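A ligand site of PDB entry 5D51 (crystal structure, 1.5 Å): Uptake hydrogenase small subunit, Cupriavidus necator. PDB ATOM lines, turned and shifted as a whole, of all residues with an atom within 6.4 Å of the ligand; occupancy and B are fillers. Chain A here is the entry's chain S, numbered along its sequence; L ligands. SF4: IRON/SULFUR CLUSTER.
Arg 192 touches the ligand.
Phe 196 touches the ligand (CB to S1, 3.9 Å).
Tyr 217 touches the ligand.
CA of Gly 223 touches S2 of the ligand, at 3.8 Å.
Pro 224 touches the ligand (CD to S3, 3.9 Å).
Ile 243 touches the ligand (CG2 to S4, 3.7 Å).
Hydrophobic or aromatic side chains within 4 Å of the ligand: His 187, Phe 196, Leu 216, Tyr 217, Pro 224 and Ile 243.
The nearest printed residue that does not touch the ligand is Ile 186 (4.1 Å).
FE4 of the ligand is bound by ND1 of His 187 (2.1 Å).
FE2 of the ligand is bound by SG of Cys 215 (2.3 Å).
SG of Cys 221 is bound to FE1 of the ligand (2.3 Å).
An iron atom (FE3) of the ligand is bound by the side-chain sulfur of Cys 190.
The backbone NH of Leu 216 lies close to a sulfur (S4) of the ligand, at 3.4 Å.
A sulfur (S1) of the ligand sits close to the backbone NH (N) of Arg 193 (3.6 Å).
The backbone carbonyl oxygen of His 187 is in hydrogen-bond range of the guanidinium group of Arg 193 (3.0 Å).
O of Gly 223 sits at hydrogen-bond distance from N of His 187 (3.3 Å).
The backbone carbonyl oxygen (O) of Leu 216 sits at hydrogen-bond distance from the backbone NH (N) of Cys 221 (3.2 Å).
N of Cys 249 lies close to SG of Cys 221.
SG of Cys 190 sits close to N of Arg 192, at 3.5 Å.
O of Ile 243 sits at hydrogen-bond distance from NH2 of Arg 192 (3.0 Å).
The backbone carbonyl oxygen (O) of Phe 214 sits at hydrogen-bond distance from the guanidinium group (NH1) of Arg 192 (2.7 Å).
The side-chain hydroxyl (OH) of Tyr 191 is in hydrogen-bond range of the guanidinium group (NE) of Arg 192, 3.0 Å away.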
ATOM      1  N   ILE A 186      -2.621   6.932 -12.968  1.00  0.00           N
ATOM      2  CA  ILE A 186      -2.444   8.382 -13.022  1.00  0.00           C
ATOM      3  C   ILE A 186      -3.591   9.055 -12.252  1.00  0.00           C
ATOM      4  O   ILE A 186      -3.370   9.973 -11.469  1.00  0.00           O
ATOM      5  CB  ILE A 186      -2.447   8.919 -14.482  1.00  0.00           C
ATOM      6  CG1 ILE A 186      -1.380   8.254 -15.360  1.00  0.00           C
ATOM      7  CG2 ILE A 186      -2.268  10.433 -14.539  1.00  0.00           C
ATOM      8  CD1 ILE A 186       0.023   8.317 -14.814  1.00  0.00           C
ATOM      9  N   HIS A 187      -4.781   8.543 -12.472  1.00  0.00           N
ATOM     10  CA  HIS A 187      -6.037   9.075 -11.936  1.00  0.00           C
ATOM     11  C   HIS A 187      -6.125   9.031 -10.402  1.00  0.00           C
ATOM     12  O   HIS A 187      -6.851   9.780  -9.841  1.00  0.00           O
ATOM     13  CB  HIS A 187      -7.169   8.298 -12.596  1.00  0.00           C
ATOM     14  CG  HIS A 187      -8.548   8.766 -12.262  1.00  0.00           C
ATOM     15  ND1 HIS A 187      -9.093   9.879 -12.811  1.00  0.00           N
ATOM     16  CD2 HIS A 187      -9.511   8.210 -11.493  1.00  0.00           C
ATOM     17  CE1 HIS A 187     -10.332  10.018 -12.379  1.00  0.00           C
ATOM     18  NE2 HIS A 187     -10.599   9.037 -11.554  1.00  0.00           N
ATOM     19  N   ASP A 188      -5.376   8.144  -9.753  1.00  0.00           N
ATOM     20  CA  ASP A 188      -5.387   8.016  -8.288  1.00  0.00           C
ATOM     21  C   ASP A 188      -5.029   9.328  -7.578  1.00  0.00           C
ATOM     22  O   ASP A 188      -5.754   9.767  -6.689  1.00  0.00           O
ATOM     23  CB  ASP A 188      -4.434   6.900  -7.797  1.00  0.00           C
ATOM     24  CG  ASP A 188      -4.857   5.486  -8.236  1.00  0.00           C
ATOM     25  OD1 ASP A 188      -6.021   5.298  -8.616  1.00  0.00           O
ATOM     26  OD2 ASP A 188      -4.002   4.566  -8.191  1.00  0.00           O
ATOM     27  N   CYS A 190      -3.828  12.277  -9.435  1.00  0.00           N
ATOM     28  CA  CYS A 190      -3.897  13.425 -10.340  1.00  0.00           C
ATOM     29  C   CYS A 190      -4.504  14.628  -9.621  1.00  0.00           C
ATOM     30  O   CYS A 190      -5.567  14.512  -9.032  1.00  0.00           O
ATOM     31  CB  CYS A 190      -4.744  13.099 -11.566  1.00  0.00           C
ATOM     32  SG  CYS A 190      -4.947  14.481 -12.711  1.00  0.00           S
ATOM     33  N   TYR A 191      -3.820  15.774  -9.673  1.00  0.00           N
ATOM     34  CA  TYR A 191      -4.281  16.975  -8.975  1.00  0.00           C
ATOM     35  C   TYR A 191      -5.627  17.504  -9.496  1.00  0.00           C
ATOM     36  O   TYR A 191      -6.273  18.273  -8.804  1.00  0.00           O
ATOM     37  CB  TYR A 191      -3.230  18.093  -9.027  1.00  0.00           C
ATOM     38  CG  TYR A 191      -3.223  18.865 -10.335  1.00  0.00           C
ATOM     39  CD1 TYR A 191      -2.689  18.300 -11.501  1.00  0.00           C
ATOM     40  CD2 TYR A 191      -3.758  20.134 -10.416  1.00  0.00           C
ATOM     41  CE1 TYR A 191      -2.698  18.990 -12.702  1.00  0.00           C
ATOM     42  CE2 TYR A 191      -3.764  20.834 -11.609  1.00  0.00           C
ATOM     43  CZ  TYR A 191      -3.224  20.257 -12.747  1.00  0.00           C
ATOM     44  OH  TYR A 191      -3.239  20.950 -13.927  1.00  0.00           O
ATOM     45  N   ARG A 192      -6.046  17.100 -10.699  1.00  0.00           N
ATOM     46  CA  ARG A 192      -7.375  17.482 -11.242  1.00  0.00           C
ATOM     47  C   ARG A 192      -8.521  16.563 -10.759  1.00  0.00           C
ATOM     48  O   ARG A 192      -9.672  16.780 -11.124  1.00  0.00           O
ATOM     49  CB  ARG A 192      -7.344  17.516 -12.768  1.00  0.00           C
ATOM     50  CG  ARG A 192      -6.328  18.485 -13.326  1.00  0.00           C
ATOM     51  CD  ARG A 192      -6.620  18.832 -14.771  1.00  0.00           C
ATOM     52  NE  ARG A 192      -5.591  19.731 -15.296  1.00  0.00           N
ATOM     53  CZ  ARG A 192      -5.745  20.542 -16.346  1.00  0.00           C
ATOM     54  NH1 ARG A 192      -6.890  20.617 -17.020  1.00  0.00           N
ATOM     55  NH2 ARG A 192      -4.726  21.308 -16.725  1.00  0.00           N
ATOM     56  N   ARG A 193      -8.201  15.556  -9.961  1.00  0.00           N
ATOM     57  CA  ARG A 193      -9.195  14.586  -9.459  1.00  0.00           C
ATOM     58  C   ARG A 193     -10.388  15.205  -8.697  1.00  0.00           C
ATOM     59  O   ARG A 193     -11.522  14.765  -8.899  1.00  0.00           O
ATOM     60  CB  ARG A 193      -8.480  13.521  -8.604  1.00  0.00           C
ATOM     61  CG  ARG A 193      -9.357  12.419  -8.020  1.00  0.00           C
ATOM     62  CD  ARG A 193     -10.014  11.578  -9.106  1.00  0.00           C
ATOM     63  NE  ARG A 193     -10.878  10.567  -8.493  1.00  0.00           N
ATOM     64  CZ  ARG A 193     -10.489   9.369  -8.079  1.00  0.00           C
ATOM     65  NH1 ARG A 193      -9.216   8.963  -8.206  1.00  0.00           N
ATOM     66  NH2 ARG A 193     -11.383   8.540  -7.536  1.00  0.00           N
ATOM     67  N   PRO A 194     -10.150  16.218  -7.841  1.00  0.00           N
ATOM     68  CA  PRO A 194     -11.317  16.866  -7.225  1.00  0.00           C
ATOM     69  C   PRO A 194     -12.319  17.417  -8.257  1.00  0.00           C
ATOM     70  O   PRO A 194     -13.523  17.402  -8.017  1.00  0.00           O
ATOM     71  CB  PRO A 194     -10.692  17.993  -6.386  1.00  0.00           C
ATOM     72  CG  PRO A 194      -9.339  17.457  -6.043  1.00  0.00           C
ATOM     73  CD  PRO A 194      -8.888  16.736  -7.286  1.00  0.00           C
ATOM     74  N   HIS A 195     -11.822  17.892  -9.407  1.00  0.00           N
ATOM     75  CA  HIS A 195     -12.716  18.329 -10.479  1.00  0.00           C
ATOM     76  C   HIS A 195     -13.479  17.151 -11.079  1.00  0.00           C
ATOM     77  O   HIS A 195     -14.689  17.234 -11.289  1.00  0.00           O
ATOM     78  CB  HIS A 195     -11.960  19.098 -11.568  1.00  0.00           C
ATOM     79  CG  HIS A 195     -11.429  20.417 -11.097  1.00  0.00           C
ATOM     80  ND1 HIS A 195     -12.250  21.396 -10.586  1.00  0.00           N
ATOM     81  CD2 HIS A 195     -10.174  20.914 -11.050  1.00  0.00           C
ATOM     82  CE1 HIS A 195     -11.519  22.439 -10.256  1.00  0.00           C
ATOM     83  NE2 HIS A 195     -10.258  22.174 -10.523  1.00  0.00           N
ATOM     84  N   PHE A 196     -12.763  16.047 -11.345  1.00  0.00           N
ATOM     85  CA  PHE A 196     -13.415  14.813 -11.795  1.00  0.00           C
ATOM     86  C   PHE A 196     -14.524  14.405 -10.838  1.00  0.00           C
ATOM     87  O   PHE A 196     -15.645  14.106 -11.264  1.00  0.00           O
ATOM     88  CB  PHE A 196     -12.420  13.678 -11.892  1.00  0.00           C
ATOM     89  CG  PHE A 196     -13.034  12.367 -12.286  1.00  0.00           C
ATOM     90  CD1 PHE A 196     -13.136  12.011 -13.625  1.00  0.00           C
ATOM     91  CD2 PHE A 196     -13.513  11.482 -11.327  1.00  0.00           C
ATOM     92  CE1 PHE A 196     -13.703  10.800 -14.000  1.00  0.00           C
ATOM     93  CE2 PHE A 196     -14.084  10.276 -11.695  1.00  0.00           C
ATOM     94  CZ  PHE A 196     -14.171   9.933 -13.031  1.00  0.00           C
ATOM     95  N   PHE A 201     -15.518  19.326 -15.953  1.00  0.00           N
ATOM     96  CA  PHE A 201     -14.752  18.871 -17.103  1.00  0.00           C
ATOM     97  C   PHE A 201     -14.540  19.923 -18.178  1.00  0.00           C
ATOM     98  O   PHE A 201     -15.414  20.762 -18.438  1.00  0.00           O
ATOM     99  CB  PHE A 201     -15.478  17.693 -17.777  1.00  0.00           C
ATOM    100  CG  PHE A 201     -15.730  16.545 -16.862  1.00  0.00           C
ATOM    101  CD1 PHE A 201     -14.701  15.684 -16.503  1.00  0.00           C
ATOM    102  CD2 PHE A 201     -17.008  16.296 -16.361  1.00  0.00           C
ATOM    103  CE1 PHE A 201     -14.931  14.616 -15.645  1.00  0.00           C
ATOM    104  CE2 PHE A 201     -17.244  15.222 -15.518  1.00  0.00           C
ATOM    105  CZ  PHE A 201     -16.203  14.380 -15.163  1.00  0.00           C
ATOM    106  N   PHE A 214      -9.852  22.243 -15.151  1.00  0.00           N
ATOM    107  CA  PHE A 214     -10.848  21.188 -14.946  1.00  0.00           C
ATOM    108  C   PHE A 214     -10.361  19.865 -15.521  1.00  0.00           C
ATOM    109  O   PHE A 214      -9.426  19.815 -16.342  1.00  0.00           O
ATOM    110  CB  PHE A 214     -12.218  21.599 -15.541  1.00  0.00           C
ATOM    111  CG  PHE A 214     -13.040  22.519 -14.643  1.00  0.00           C
ATOM    112  CD1 PHE A 214     -12.488  23.179 -13.531  1.00  0.00           C
ATOM    113  CD2 PHE A 214     -14.376  22.763 -14.947  1.00  0.00           C
ATOM    114  CE1 PHE A 214     -13.263  24.009 -12.733  1.00  0.00           C
ATOM    115  CE2 PHE A 214     -15.146  23.606 -14.156  1.00  0.00           C
ATOM    116  CZ  PHE A 214     -14.588  24.226 -13.052  1.00  0.00           C
ATOM    117  N   CYS A 215     -10.991  18.784 -15.075  1.00  0.00           N
ATOM    118  CA  CYS A 215     -10.611  17.433 -15.478  1.00  0.00           C
ATOM    119  C   CYS A 215     -10.698  17.240 -16.995  1.00  0.00           C
ATOM    120  O   CYS A 215     -11.599  17.785 -17.662  1.00  0.00           O
ATOM    121  CB  CYS A 215     -11.480  16.403 -14.738  1.00  0.00           C
ATOM    122  SG  CYS A 215     -11.295  14.717 -15.326  1.00  0.00           S
ATOM    123  N   LEU A 216      -9.748  16.461 -17.529  1.00  0.00           N
ATOM    124  CA  LEU A 216      -9.606  16.223 -18.977  1.00  0.00           C
ATOM    125  C   LEU A 216     -10.246  14.935 -19.479  1.00  0.00           C
ATOM    126  O   LEU A 216     -10.057  14.567 -20.653  1.00  0.00           O
ATOM    127  CB  LEU A 216      -8.121  16.268 -19.365  1.00  0.00           C
ATOM    128  CG  LEU A 216      -7.486  17.648 -19.135  1.00  0.00           C
ATOM    129  CD1 LEU A 216      -5.963  17.573 -19.164  1.00  0.00           C
ATOM    130  CD2 LEU A 216      -7.982  18.649 -20.171  1.00  0.00           C
ATOM    131  N   TYR A 217     -11.032  14.267 -18.628  1.00  0.00           N
ATOM    132  CA  TYR A 217     -11.685  12.998 -18.981  1.00  0.00           C
ATOM    133  C   TYR A 217     -12.463  13.074 -20.294  1.00  0.00           C
ATOM    134  O   TYR A 217     -12.352  12.191 -21.162  1.00  0.00           O
ATOM    135  CB  TYR A 217     -12.632  12.547 -17.861  1.00  0.00           C
ATOM    136  CG  TYR A 217     -13.265  11.188 -18.046  1.00  0.00           C
ATOM    137  CD1 TYR A 217     -12.632  10.045 -17.583  1.00  0.00           C
ATOM    138  CD2 TYR A 217     -14.510  11.050 -18.652  1.00  0.00           C
ATOM    139  CE1 TYR A 217     -13.212   8.790 -17.734  1.00  0.00           C
ATOM    140  CE2 TYR A 217     -15.101   9.795 -18.812  1.00  0.00           C
ATOM    141  CZ  TYR A 217     -14.440   8.666 -18.352  1.00  0.00           C
ATOM    142  OH  TYR A 217     -15.025   7.416 -18.497  1.00  0.00           O
ATOM    143  N   LYS A 218     -13.263  14.126 -20.453  1.00  0.00           N
ATOM    144  CA  LYS A 218     -14.113  14.255 -21.656  1.00  0.00           C
ATOM    145  C   LYS A 218     -13.328  14.676 -22.901  1.00  0.00           C
ATOM    146  O   LYS A 218     -13.876  14.647 -24.013  1.00  0.00           O
ATOM    147  CB  LYS A 218     -15.289  15.196 -21.391  1.00  0.00           C
ATOM    148  CG  LYS A 218     -16.206  14.634 -20.311  1.00  0.00           C
ATOM    149  CD  LYS A 218     -17.475  15.466 -20.134  1.00  0.00           C
ATOM    150  CE  LYS A 218     -18.425  14.760 -19.188  1.00  0.00           C
ATOM    151  NZ  LYS A 218     -19.676  15.526 -18.964  1.00  0.00           N
ATOM    152  N   CYS A 221      -8.745  11.855 -21.752  1.00  0.00           N
ATOM    153  CA  CYS A 221      -7.698  11.474 -20.796  1.00  0.00           C
ATOM    154  C   CYS A 221      -7.806   9.992 -20.452  1.00  0.00           C
ATOM    155  O   CYS A 221      -8.862   9.511 -20.036  1.00  0.00           O
ATOM    156  CB  CYS A 221      -7.775  12.317 -19.528  1.00  0.00           C
ATOM    157  SG  CYS A 221      -6.424  11.932 -18.363  1.00  0.00           S
ATOM    158  N   LYS A 222      -6.710   9.268 -20.633  1.00  0.00           N
ATOM    159  CA  LYS A 222      -6.643   7.832 -20.325  1.00  0.00           C
ATOM    160  C   LYS A 222      -6.001   7.560 -18.953  1.00  0.00           C
ATOM    161  O   LYS A 222      -5.667   6.415 -18.620  1.00  0.00           O
ATOM    162  CB  LYS A 222      -5.947   7.071 -21.460  1.00  0.00           C
ATOM    163  CG  LYS A 222      -6.640   7.242 -22.808  1.00  0.00           C
ATOM    164  CD  LYS A 222      -8.152   7.011 -22.707  1.00  0.00           C
ATOM    165  CE  LYS A 222      -8.870   6.901 -24.041  1.00  0.00           C
ATOM    166  NZ  LYS A 222      -8.631   8.065 -24.949  1.00  0.00           N
ATOM    167  N   GLY A 223      -5.873   8.604 -18.128  1.00  0.00           N
ATOM    168  CA  GLY A 223      -5.367   8.476 -16.775  1.00  0.00           C
ATOM    169  C   GLY A 223      -6.066   7.418 -15.920  1.00  0.00           C
ATOM    170  O   GLY A 223      -5.397   6.737 -15.137  1.00  0.00           O
ATOM    171  N   PRO A 224      -7.401   7.269 -16.052  1.00  0.00           N
ATOM    172  CA  PRO A 224      -8.084   6.250 -15.243  1.00  0.00           C
ATOM    173  C   PRO A 224      -7.710   4.797 -15.504  1.00  0.00           C
ATOM    174  O   PRO A 224      -8.017   3.947 -14.674  1.00  0.00           O
ATOM    175  CB  PRO A 224      -9.573   6.481 -15.564  1.00  0.00           C
ATOM    176  CG  PRO A 224      -9.639   7.916 -15.957  1.00  0.00           C
ATOM    177  CD  PRO A 224      -8.370   8.164 -16.723  1.00  0.00           C
ATOM    178  N   PHE A 241       3.553  17.462 -15.884  1.00  0.00           N
ATOM    179  CA  PHE A 241       3.205  16.203 -16.525  1.00  0.00           C
ATOM    180  C   PHE A 241       2.120  16.501 -17.562  1.00  0.00           C
ATOM    181  O   PHE A 241       1.600  17.611 -17.589  1.00  0.00           O
ATOM    182  CB  PHE A 241       2.889  15.069 -15.523  1.00  0.00           C
ATOM    183  CG  PHE A 241       1.562  15.152 -14.811  1.00  0.00           C
ATOM    184  CD1 PHE A 241       1.302  16.189 -13.919  1.00  0.00           C
ATOM    185  CD2 PHE A 241       0.608  14.151 -14.991  1.00  0.00           C
ATOM    186  CE1 PHE A 241       0.090  16.227 -13.235  1.00  0.00           C
ATOM    187  CE2 PHE A 241      -0.596  14.196 -14.305  1.00  0.00           C
ATOM    188  CZ  PHE A 241      -0.855  15.233 -13.427  1.00  0.00           C
ATOM    189  N   ILE A 243      -1.045  16.111 -18.045  1.00  0.00           N
ATOM    190  CA  ILE A 243      -2.298  16.680 -17.549  1.00  0.00           C
ATOM    191  C   ILE A 243      -2.102  18.079 -16.978  1.00  0.00           C
ATOM    192  O   ILE A 243      -2.925  18.967 -17.236  1.00  0.00           O
ATOM    193  CB  ILE A 243      -2.959  15.707 -16.543  1.00  0.00           C
ATOM    194  CG1 ILE A 243      -3.499  14.494 -17.329  1.00  0.00           C
ATOM    195  CG2 ILE A 243      -4.061  16.398 -15.738  1.00  0.00           C
ATOM    196  CD1 ILE A 243      -3.461  13.185 -16.559  1.00  0.00           C
ATOM    197  N   GLY A 248      -4.759  15.529 -22.038  1.00  0.00           N
ATOM    198  CA  GLY A 248      -5.035  14.279 -21.367  1.00  0.00           C
ATOM    199  C   GLY A 248      -3.898  13.273 -21.541  1.00  0.00           C
ATOM    200  O   GLY A 248      -3.156  13.303 -22.518  1.00  0.00           O
ATOM    201  N   CYS A 249      -3.746  12.396 -20.560  1.00  0.00           N
ATOM    202  CA  CYS A 249      -2.915  11.222 -20.720  1.00  0.00           C
ATOM    203  C   CYS A 249      -3.408  10.463 -21.961  1.00  0.00           C
ATOM    204  O   CYS A 249      -4.621  10.338 -22.178  1.00  0.00           O
ATOM    205  CB  CYS A 249      -3.025  10.360 -19.450  1.00  0.00           C
ATOM    206  SG  CYS A 249      -2.184   8.773 -19.488  1.00  0.00           S
HETATM  207 FE1  SF4 L   1      -7.329  12.486 -16.323  1.00  0.00          FE
HETATM  208 FE2  SF4 L   1      -9.245  13.831 -14.894  1.00  0.00          FE
HETATM  209 FE3  SF4 L   1      -6.711  13.607 -13.918  1.00  0.00          FE
HETATM  210 FE4  SF4 L   1      -8.361  11.444 -13.970  1.00  0.00          FE
HETATM  211  S1  SF4 L   1      -8.636  13.379 -12.740  1.00  0.00           S
HETATM  212  S2  SF4 L   1      -6.176  11.504 -14.577  1.00  0.00           S
HETATM  213  S3  SF4 L   1      -9.460  11.791 -15.988  1.00  0.00           S
HETATM  214  S4  SF4 L   1      -7.377  14.735 -15.832  1.00  0.00           S
